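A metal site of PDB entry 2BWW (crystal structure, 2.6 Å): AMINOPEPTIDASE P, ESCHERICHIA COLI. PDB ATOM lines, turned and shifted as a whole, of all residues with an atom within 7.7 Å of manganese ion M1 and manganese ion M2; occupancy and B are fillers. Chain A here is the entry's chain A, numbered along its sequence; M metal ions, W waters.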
ATOM      1  N   TYR A 229      11.487  27.036  -7.528  1.00  0.00           N
ATOM      2  CA  TYR A 229      10.229  26.324  -7.761  1.00  0.00           C
ATOM      3  C   TYR A 229       9.260  27.275  -8.467  1.00  0.00           C
ATOM      4  O   TYR A 229       9.471  28.481  -8.488  1.00  0.00           O
ATOM      5  CB  TYR A 229       9.610  25.801  -6.437  1.00  0.00           C
ATOM      6  CG  TYR A 229       9.416  26.879  -5.402  1.00  0.00           C
ATOM      7  CD1 TYR A 229      10.413  27.177  -4.485  1.00  0.00           C
ATOM      8  CD2 TYR A 229       8.251  27.638  -5.364  1.00  0.00           C
ATOM      9  CE1 TYR A 229      10.254  28.175  -3.567  1.00  0.00           C
ATOM     10  CE2 TYR A 229       8.074  28.631  -4.419  1.00  0.00           C
ATOM     11  CZ  TYR A 229       9.082  28.905  -3.528  1.00  0.00           C
ATOM     12  OH  TYR A 229       8.937  29.899  -2.586  1.00  0.00           O
ATOM     13  N   ILE A 232       3.901  30.915  -7.069  1.00  0.00           N
ATOM     14  CA  ILE A 232       2.479  30.949  -6.767  1.00  0.00           C
ATOM     15  C   ILE A 232       2.022  32.372  -6.472  1.00  0.00           C
ATOM     16  O   ILE A 232       2.571  33.029  -5.589  1.00  0.00           O
ATOM     17  CB  ILE A 232       2.158  30.106  -5.496  1.00  0.00           C
ATOM     18  CG1 ILE A 232       2.446  28.609  -5.718  1.00  0.00           C
ATOM     19  CG2 ILE A 232       0.696  30.329  -5.042  1.00  0.00           C
ATOM     20  CD1 ILE A 232       2.492  27.799  -4.411  1.00  0.00           C
ATOM     21  N   LEU A 258      -1.810  35.629  -1.949  1.00  0.00           N
ATOM     22  CA  LEU A 258      -0.805  34.757  -1.326  1.00  0.00           C
ATOM     23  C   LEU A 258       0.315  34.540  -2.347  1.00  0.00           C
ATOM     24  O   LEU A 258       0.096  33.973  -3.423  1.00  0.00           O
ATOM     25  CB  LEU A 258      -1.445  33.425  -0.967  1.00  0.00           C
ATOM     26  CG  LEU A 258      -0.626  32.332  -0.291  1.00  0.00           C
ATOM     27  CD1 LEU A 258      -1.569  31.310   0.312  1.00  0.00           C
ATOM     28  CD2 LEU A 258       0.347  31.641  -1.245  1.00  0.00           C
ATOM     29  N   ILE A 259       1.509  35.001  -1.997  1.00  0.00           N
ATOM     30  CA  ILE A 259       2.665  34.877  -2.875  1.00  0.00           C
ATOM     31  C   ILE A 259       3.686  33.962  -2.253  1.00  0.00           C
ATOM     32  O   ILE A 259       4.236  34.266  -1.183  1.00  0.00           O
ATOM     33  CB  ILE A 259       3.319  36.219  -3.167  1.00  0.00           C
ATOM     34  CG1 ILE A 259       2.285  37.154  -3.787  1.00  0.00           C
ATOM     35  CG2 ILE A 259       4.490  36.020  -4.115  1.00  0.00           C
ATOM     36  CD1 ILE A 259       2.848  38.410  -4.353  1.00  0.00           C
ATOM     37  N   ASP A 260       3.928  32.831  -2.916  1.00  0.00           N
ATOM     38  CA  ASP A 260       4.977  31.913  -2.527  1.00  0.00           C
ATOM     39  C   ASP A 260       5.971  31.835  -3.675  1.00  0.00           C
ATOM     40  O   ASP A 260       5.685  31.264  -4.728  1.00  0.00           O
ATOM     41  CB  ASP A 260       4.378  30.539  -2.207  1.00  0.00           C
ATOM     42  CG  ASP A 260       5.363  29.586  -1.535  1.00  0.00           C
ATOM     43  OD1 ASP A 260       6.565  29.863  -1.451  1.00  0.00           O
ATOM     44  OD2 ASP A 260       4.911  28.520  -1.099  1.00  0.00           O
ATOM     45  N   ALA A 261       7.137  32.455  -3.460  1.00  0.00           N
ATOM     46  CA  ALA A 261       8.216  32.471  -4.421  1.00  0.00           C
ATOM     47  C   ALA A 261       9.575  32.360  -3.748  1.00  0.00           C
ATOM     48  O   ALA A 261       9.761  32.836  -2.608  1.00  0.00           O
ATOM     49  CB  ALA A 261       8.155  33.727  -5.260  1.00  0.00           C
ATOM     50  N   GLY A 262      10.511  31.727  -4.454  1.00  0.00           N
ATOM     51  CA  GLY A 262      11.877  31.502  -3.952  1.00  0.00           C
ATOM     52  C   GLY A 262      12.876  31.551  -5.084  1.00  0.00           C
ATOM     53  O   GLY A 262      12.581  31.126  -6.202  1.00  0.00           O
ATOM     54  N   GLY A 270      15.798  29.607  -1.832  1.00  0.00           N
ATOM     55  CA  GLY A 270      15.000  30.412  -0.934  1.00  0.00           C
ATOM     56  C   GLY A 270      13.562  29.927  -1.050  1.00  0.00           C
ATOM     57  O   GLY A 270      13.177  29.306  -2.042  1.00  0.00           O
ATOM     58  N   ASP A 271      12.771  30.199  -0.011  1.00  0.00           N
ATOM     59  CA  ASP A 271      11.367  29.789  -0.011  1.00  0.00           C
ATOM     60  C   ASP A 271      10.576  30.635   0.989  1.00  0.00           C
ATOM     61  O   ASP A 271      10.560  30.361   2.163  1.00  0.00           O
ATOM     62  CB  ASP A 271      11.257  28.290   0.322  1.00  0.00           C
ATOM     63  CG  ASP A 271       9.839  27.783   0.298  1.00  0.00           C
ATOM     64  OD1 ASP A 271       8.939  28.560  -0.085  1.00  0.00           O
ATOM     65  OD2 ASP A 271       9.635  26.610   0.678  1.00  0.00           O
ATOM     66  N   ILE A 272       9.941  31.691   0.480  1.00  0.00           N
ATOM     67  CA  ILE A 272       9.168  32.616   1.307  1.00  0.00           C
ATOM     68  C   ILE A 272       7.734  32.646   0.808  1.00  0.00           C
ATOM     69  O   ILE A 272       7.468  32.568  -0.407  1.00  0.00           O
ATOM     70  CB  ILE A 272       9.755  34.038   1.217  1.00  0.00           C
ATOM     71  CG1 ILE A 272      11.160  34.086   1.803  1.00  0.00           C
ATOM     72  CG2 ILE A 272       8.855  35.058   1.926  1.00  0.00           C
ATOM     73  CD1 ILE A 272      11.808  35.443   1.683  1.00  0.00           C
ATOM     74  N   THR A 273       6.802  32.766   1.751  1.00  0.00           N
ATOM     75  CA  THR A 273       5.391  33.068   1.429  1.00  0.00           C
ATOM     76  C   THR A 273       4.968  34.264   2.236  1.00  0.00           C
ATOM     77  O   THR A 273       5.216  34.310   3.432  1.00  0.00           O
ATOM     78  CB  THR A 273       4.404  31.942   1.753  1.00  0.00           C
ATOM     79  OG1 THR A 273       4.888  30.674   1.257  1.00  0.00           O
ATOM     80  CG2 THR A 273       3.047  32.246   1.125  1.00  0.00           C
ATOM     81  N   GLY A 351       1.873  20.469   6.155  1.00  0.00           N
ATOM     82  CA  GLY A 351       2.769  20.404   7.303  1.00  0.00           C
ATOM     83  C   GLY A 351       3.310  21.791   7.627  1.00  0.00           C
ATOM     84  O   GLY A 351       3.129  22.725   6.852  1.00  0.00           O
ATOM     85  N   LEU A 352       3.985  21.924   8.755  1.00  0.00           N
ATOM     86  CA  LEU A 352       4.549  23.204   9.215  1.00  0.00           C
ATOM     87  C   LEU A 352       5.930  23.526   8.617  1.00  0.00           C
ATOM     88  O   LEU A 352       6.313  24.695   8.504  1.00  0.00           O
ATOM     89  CB  LEU A 352       4.660  23.183  10.741  1.00  0.00           C
ATOM     90  CG  LEU A 352       5.193  24.447  11.425  1.00  0.00           C
ATOM     91  CD1 LEU A 352       4.226  25.612  11.290  1.00  0.00           C
ATOM     92  CD2 LEU A 352       5.517  24.185  12.887  1.00  0.00           C
ATOM     93  N   SER A 353       6.693  22.485   8.269  1.00  0.00           N
ATOM     94  CA  SER A 353       8.116  22.628   7.986  1.00  0.00           C
ATOM     95  C   SER A 353       8.642  21.534   7.058  1.00  0.00           C
ATOM     96  O   SER A 353       8.242  20.379   7.125  1.00  0.00           O
ATOM     97  CB  SER A 353       8.930  22.570   9.293  1.00  0.00           C
ATOM     98  OG  SER A 353       8.639  23.682  10.149  1.00  0.00           O
ATOM     99  N   HIS A 354       9.558  21.926   6.176  1.00  0.00           N
ATOM    100  CA  HIS A 354      10.352  20.963   5.456  1.00  0.00           C
ATOM    101  C   HIS A 354      11.803  21.387   5.422  1.00  0.00           C
ATOM    102  O   HIS A 354      12.093  22.571   5.550  1.00  0.00           O
ATOM    103  CB  HIS A 354       9.821  20.760   4.040  1.00  0.00           C
ATOM    104  CG  HIS A 354       9.736  22.016   3.240  1.00  0.00           C
ATOM    105  ND1 HIS A 354      10.839  22.639   2.688  1.00  0.00           N
ATOM    106  CD2 HIS A 354       8.661  22.741   2.845  1.00  0.00           C
ATOM    107  CE1 HIS A 354      10.446  23.714   2.020  1.00  0.00           C
ATOM    108  NE2 HIS A 354       9.128  23.796   2.091  1.00  0.00           N
ATOM    109  N   TRP A 355      12.702  20.427   5.263  1.00  0.00           N
ATOM    110  CA  TRP A 355      14.099  20.726   5.068  1.00  0.00           C
ATOM    111  C   TRP A 355      14.266  21.642   3.849  1.00  0.00           C
ATOM    112  O   TRP A 355      13.512  21.568   2.877  1.00  0.00           O
ATOM    113  CB  TRP A 355      14.917  19.444   4.843  1.00  0.00           C
ATOM    114  CG  TRP A 355      14.778  18.349   5.893  1.00  0.00           C
ATOM    115  CD1 TRP A 355      14.545  17.035   5.654  1.00  0.00           C
ATOM    116  CD2 TRP A 355      14.872  18.491   7.304  1.00  0.00           C
ATOM    117  NE1 TRP A 355      14.485  16.344   6.825  1.00  0.00           N
ATOM    118  CE2 TRP A 355      14.678  17.217   7.862  1.00  0.00           C
ATOM    119  CE3 TRP A 355      15.078  19.582   8.150  1.00  0.00           C
ATOM    120  CZ2 TRP A 355      14.701  16.995   9.254  1.00  0.00           C
ATOM    121  CZ3 TRP A 355      15.106  19.355   9.530  1.00  0.00           C
ATOM    122  CH2 TRP A 355      14.923  18.071  10.063  1.00  0.00           C
ATOM    123  N   LEU A 356      15.274  22.506   3.905  1.00  0.00           N
ATOM    124  CA  LEU A 356      15.580  23.407   2.801  1.00  0.00           C
ATOM    125  C   LEU A 356      17.072  23.309   2.465  1.00  0.00           C
ATOM    126  O   LEU A 356      17.901  23.185   3.345  1.00  0.00           O
ATOM    127  CB  LEU A 356      15.222  24.832   3.187  1.00  0.00           C
ATOM    128  CG  LEU A 356      15.280  25.914   2.116  1.00  0.00           C
ATOM    129  CD1 LEU A 356      14.202  25.705   1.078  1.00  0.00           C
ATOM    130  CD2 LEU A 356      15.155  27.286   2.771  1.00  0.00           C
ATOM    131  N   VAL A 360      14.341  22.764  -2.746  1.00  0.00           N
ATOM    132  CA  VAL A 360      13.407  23.485  -1.878  1.00  0.00           C
ATOM    133  C   VAL A 360      12.778  22.526  -0.863  1.00  0.00           C
ATOM    134  O   VAL A 360      12.740  22.814   0.334  1.00  0.00           O
ATOM    135  CB  VAL A 360      12.344  24.298  -2.673  1.00  0.00           C
ATOM    136  CG1 VAL A 360      11.475  23.410  -3.515  1.00  0.00           C
ATOM    137  CG2 VAL A 360      11.480  25.128  -1.723  1.00  0.00           C
ATOM    138  N   HIS A 361      12.315  21.370  -1.323  1.00  0.00           N
ATOM    139  CA  HIS A 361      11.907  20.287  -0.433  1.00  0.00           C
ATOM    140  C   HIS A 361      13.080  19.378  -0.250  1.00  0.00           C
ATOM    141  O   HIS A 361      13.205  18.374  -0.966  1.00  0.00           O
ATOM    142  CB  HIS A 361      10.733  19.514  -1.016  1.00  0.00           C
ATOM    143  CG  HIS A 361       9.478  20.315  -1.083  1.00  0.00           C
ATOM    144  ND1 HIS A 361       8.390  19.937  -1.834  1.00  0.00           N
ATOM    145  CD2 HIS A 361       9.144  21.502  -0.506  1.00  0.00           C
ATOM    146  CE1 HIS A 361       7.429  20.842  -1.695  1.00  0.00           C
ATOM    147  NE2 HIS A 361       7.866  21.798  -0.901  1.00  0.00           N
ATOM    148  N   LEU A 380      15.444  24.733   7.628  1.00  0.00           N
ATOM    149  CA  LEU A 380      14.047  24.384   7.433  1.00  0.00           C
ATOM    150  C   LEU A 380      13.115  25.598   7.309  1.00  0.00           C
ATOM    151  O   LEU A 380      13.470  26.720   7.696  1.00  0.00           O
ATOM    152  CB  LEU A 380      13.556  23.454   8.553  1.00  0.00           C
ATOM    153  CG  LEU A 380      13.615  23.986   9.986  1.00  0.00           C
ATOM    154  CD1 LEU A 380      12.605  23.248  10.855  1.00  0.00           C
ATOM    155  CD2 LEU A 380      15.022  23.878  10.563  1.00  0.00           C
ATOM    156  N   THR A 381      11.944  25.329   6.758  1.00  0.00           N
ATOM    157  CA  THR A 381      10.907  26.336   6.608  1.00  0.00           C
ATOM    158  C   THR A 381       9.941  26.289   7.778  1.00  0.00           C
ATOM    159  O   THR A 381       9.802  25.258   8.440  1.00  0.00           O
ATOM    160  CB  THR A 381      10.123  26.142   5.320  1.00  0.00           C
ATOM    161  OG1 THR A 381       9.393  24.900   5.381  1.00  0.00           O
ATOM    162  CG2 THR A 381      11.078  26.126   4.137  1.00  0.00           C
ATOM    163  N   VAL A 382       9.318  27.425   8.048  1.00  0.00           N
ATOM    164  CA  VAL A 382       8.245  27.522   9.022  1.00  0.00           C
ATOM    165  C   VAL A 382       7.099  28.168   8.269  1.00  0.00           C
ATOM    166  O   VAL A 382       7.197  29.338   7.886  1.00  0.00           O
ATOM    167  CB  VAL A 382       8.648  28.361  10.253  1.00  0.00           C
ATOM    168  CG1 VAL A 382       7.643  28.141  11.380  1.00  0.00           C
ATOM    169  CG2 VAL A 382      10.063  27.991  10.728  1.00  0.00           C
ATOM    170  N   GLU A 383       6.030  27.418   8.033  1.00  0.00           N
ATOM    171  CA  GLU A 383       5.017  27.884   7.089  1.00  0.00           C
ATOM    172  C   GLU A 383       3.581  27.497   7.460  1.00  0.00           C
ATOM    173  O   GLU A 383       2.915  26.770   6.721  1.00  0.00           O
ATOM    174  CB  GLU A 383       5.383  27.390   5.674  1.00  0.00           C
ATOM    175  CG  GLU A 383       5.590  25.877   5.531  1.00  0.00           C
ATOM    176  CD  GLU A 383       5.967  25.477   4.114  1.00  0.00           C
ATOM    177  OE1 GLU A 383       5.153  25.717   3.184  1.00  0.00           O
ATOM    178  OE2 GLU A 383       7.091  24.942   3.933  1.00  0.00           O
ATOM    179  N   ARG A 404      -1.043  32.073   4.018  1.00  0.00           N
ATOM    180  CA  ARG A 404       0.174  31.415   4.512  1.00  0.00           C
ATOM    181  C   ARG A 404       1.253  32.448   4.725  1.00  0.00           C
ATOM    182  O   ARG A 404       1.371  33.397   3.948  1.00  0.00           O
ATOM    183  CB  ARG A 404       0.651  30.364   3.528  1.00  0.00           C
ATOM    184  CG  ARG A 404       1.963  29.689   3.921  1.00  0.00           C
ATOM    185  CD  ARG A 404       2.214  28.401   3.120  1.00  0.00           C
ATOM    186  NE  ARG A 404       2.464  28.636   1.700  1.00  0.00           N
ATOM    187  CZ  ARG A 404       1.633  28.334   0.707  1.00  0.00           C
ATOM    188  NH1 ARG A 404       0.433  27.805   0.932  1.00  0.00           N
ATOM    189  NH2 ARG A 404       1.992  28.572  -0.546  1.00  0.00           N
ATOM    190  N   GLU A 406       5.424  32.210   5.405  1.00  0.00           N
ATOM    191  CA  GLU A 406       6.529  31.255   5.422  1.00  0.00           C
ATOM    192  C   GLU A 406       7.866  31.982   5.535  1.00  0.00           C
ATOM    193  O   GLU A 406       8.115  32.934   4.804  1.00  0.00           O
ATOM    194  CB  GLU A 406       6.485  30.380   4.162  1.00  0.00           C
ATOM    195  CG  GLU A 406       7.757  29.572   3.877  1.00  0.00           C
ATOM    196  CD  GLU A 406       7.561  28.519   2.798  1.00  0.00           C
ATOM    197  OE1 GLU A 406       6.719  28.753   1.899  1.00  0.00           O
ATOM    198  OE2 GLU A 406       8.260  27.470   2.837  1.00  0.00           O
ATOM    199  N   ASP A 407       8.686  31.531   6.489  1.00  0.00           N
ATOM    200  CA  ASP A 407      10.043  31.998   6.700  1.00  0.00           C
ATOM    201  C   ASP A 407      11.000  30.805   6.654  1.00  0.00           C
ATOM    202  O   ASP A 407      10.580  29.654   6.868  1.00  0.00           O
ATOM    203  CB  ASP A 407      10.174  32.678   8.070  1.00  0.00           C
ATOM    204  CG  ASP A 407       9.933  34.193   8.017  1.00  0.00           C
ATOM    205  OD1 ASP A 407      10.056  34.792   6.935  1.00  0.00           O
ATOM    206  OD2 ASP A 407       9.653  34.791   9.081  1.00  0.00           O
ATOM    207  N   ASP A 408      12.280  31.083   6.393  1.00  0.00           N
ATOM    208  CA  ASP A 408      13.342  30.066   6.344  1.00  0.00           C
ATOM    209  C   ASP A 408      14.290  30.284   7.520  1.00  0.00           C
ATOM    210  O   ASP A 408      14.733  31.421   7.782  1.00  0.00           O
ATOM    211  CB  ASP A 408      14.126  30.154   5.030  1.00  0.00           C
ATOM    212  CG  ASP A 408      13.232  30.079   3.777  1.00  0.00           C
ATOM    213  OD1 ASP A 408      12.112  29.510   3.831  1.00  0.00           O
ATOM    214  OD2 ASP A 408      13.652  30.615   2.732  1.00  0.00           O
HETATM  215 MN    MN M   1       8.092  25.659   1.844  1.00  0.00          MN
HETATM  216 MN    MN M   2       6.881  27.944  -0.114  1.00  0.00          MN
HETATM  217  O   HOH W   1       6.344  25.847   0.900  1.00  0.00           O
HETATM  218  O   HOH W   2       7.303  26.518  -1.870  1.00  0.00           O
HETATM  219  O   HOH W   3       7.286  24.292  -0.770  1.00  0.00           O
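The backbone carbonyl oxygen of His 354 sits at hydrogen-bond distance from the backbone NH of Thr 381 (3.0 Å). ND1 of His 354 sits close to O of Val 360 (3.0 Å). The side-chain carboxylate (OD1) of Asp 260 sits close to the side-chain hydroxyl (OH) of Tyr 229 (2.6 Å). The side-chain carboxylate (OE2) of Glu 383 sits close to the side-chain hydroxyl (OG1) of Thr 381, 2.7 Å away. O of Leu 352 lies within hydrogen-bond range of N of Glu 383. The side-chain hydroxyl (OG1) of Thr 273 lies within hydrogen-bond range of the guanidinium group (NE) of Arg 404 (3.2 Å). The side-chain hydroxyl (OH) of Tyr 229 sits at hydrogen-bond distance from the backbone NH (N) of Gly 262 (3.1 Å). The side-chain hydroxyl (OG) of Ser 353 sits at hydrogen-bond distance from the backbone carbonyl oxygen (O) of Thr 381 (2.6 Å).
Merely in contact with manganese ion M1: Thr 381. The nearest printed residue that does not touch manganese ion M1 is His 361 (4.7 Å).
Merely in contact with manganese ion M2: Thr 273 and Tyr 229. Five residues have an atom within 4 Å of manganese ion M2: Tyr 229, Asp 260, Asp 271, Thr 273 and Glu 406. The nearest printed residue that does not touch manganese ion M2 is Glu 383 (4.3 Å).
Manganese ion M1 is bound by water W1 (2.0 Å), OE2 of Glu 406 (2.1 Å), NE2 of His 354 (2.1 Å), OD2 of Asp 271 (2.2 Å) and OE2 of Glu 383 (2.4 Å).
Manganese ion M2 is bound by the side-chain carboxylate (OD1) of Asp 271, the side-chain carboxylate (OE1) of Glu 406, the side-chain carboxylate (OD2) of Asp 260, water W2, the side-chain carboxylate (OD1) of Asp 260 and water W1. Manganese ion M2 has six donor atoms within binding distance.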
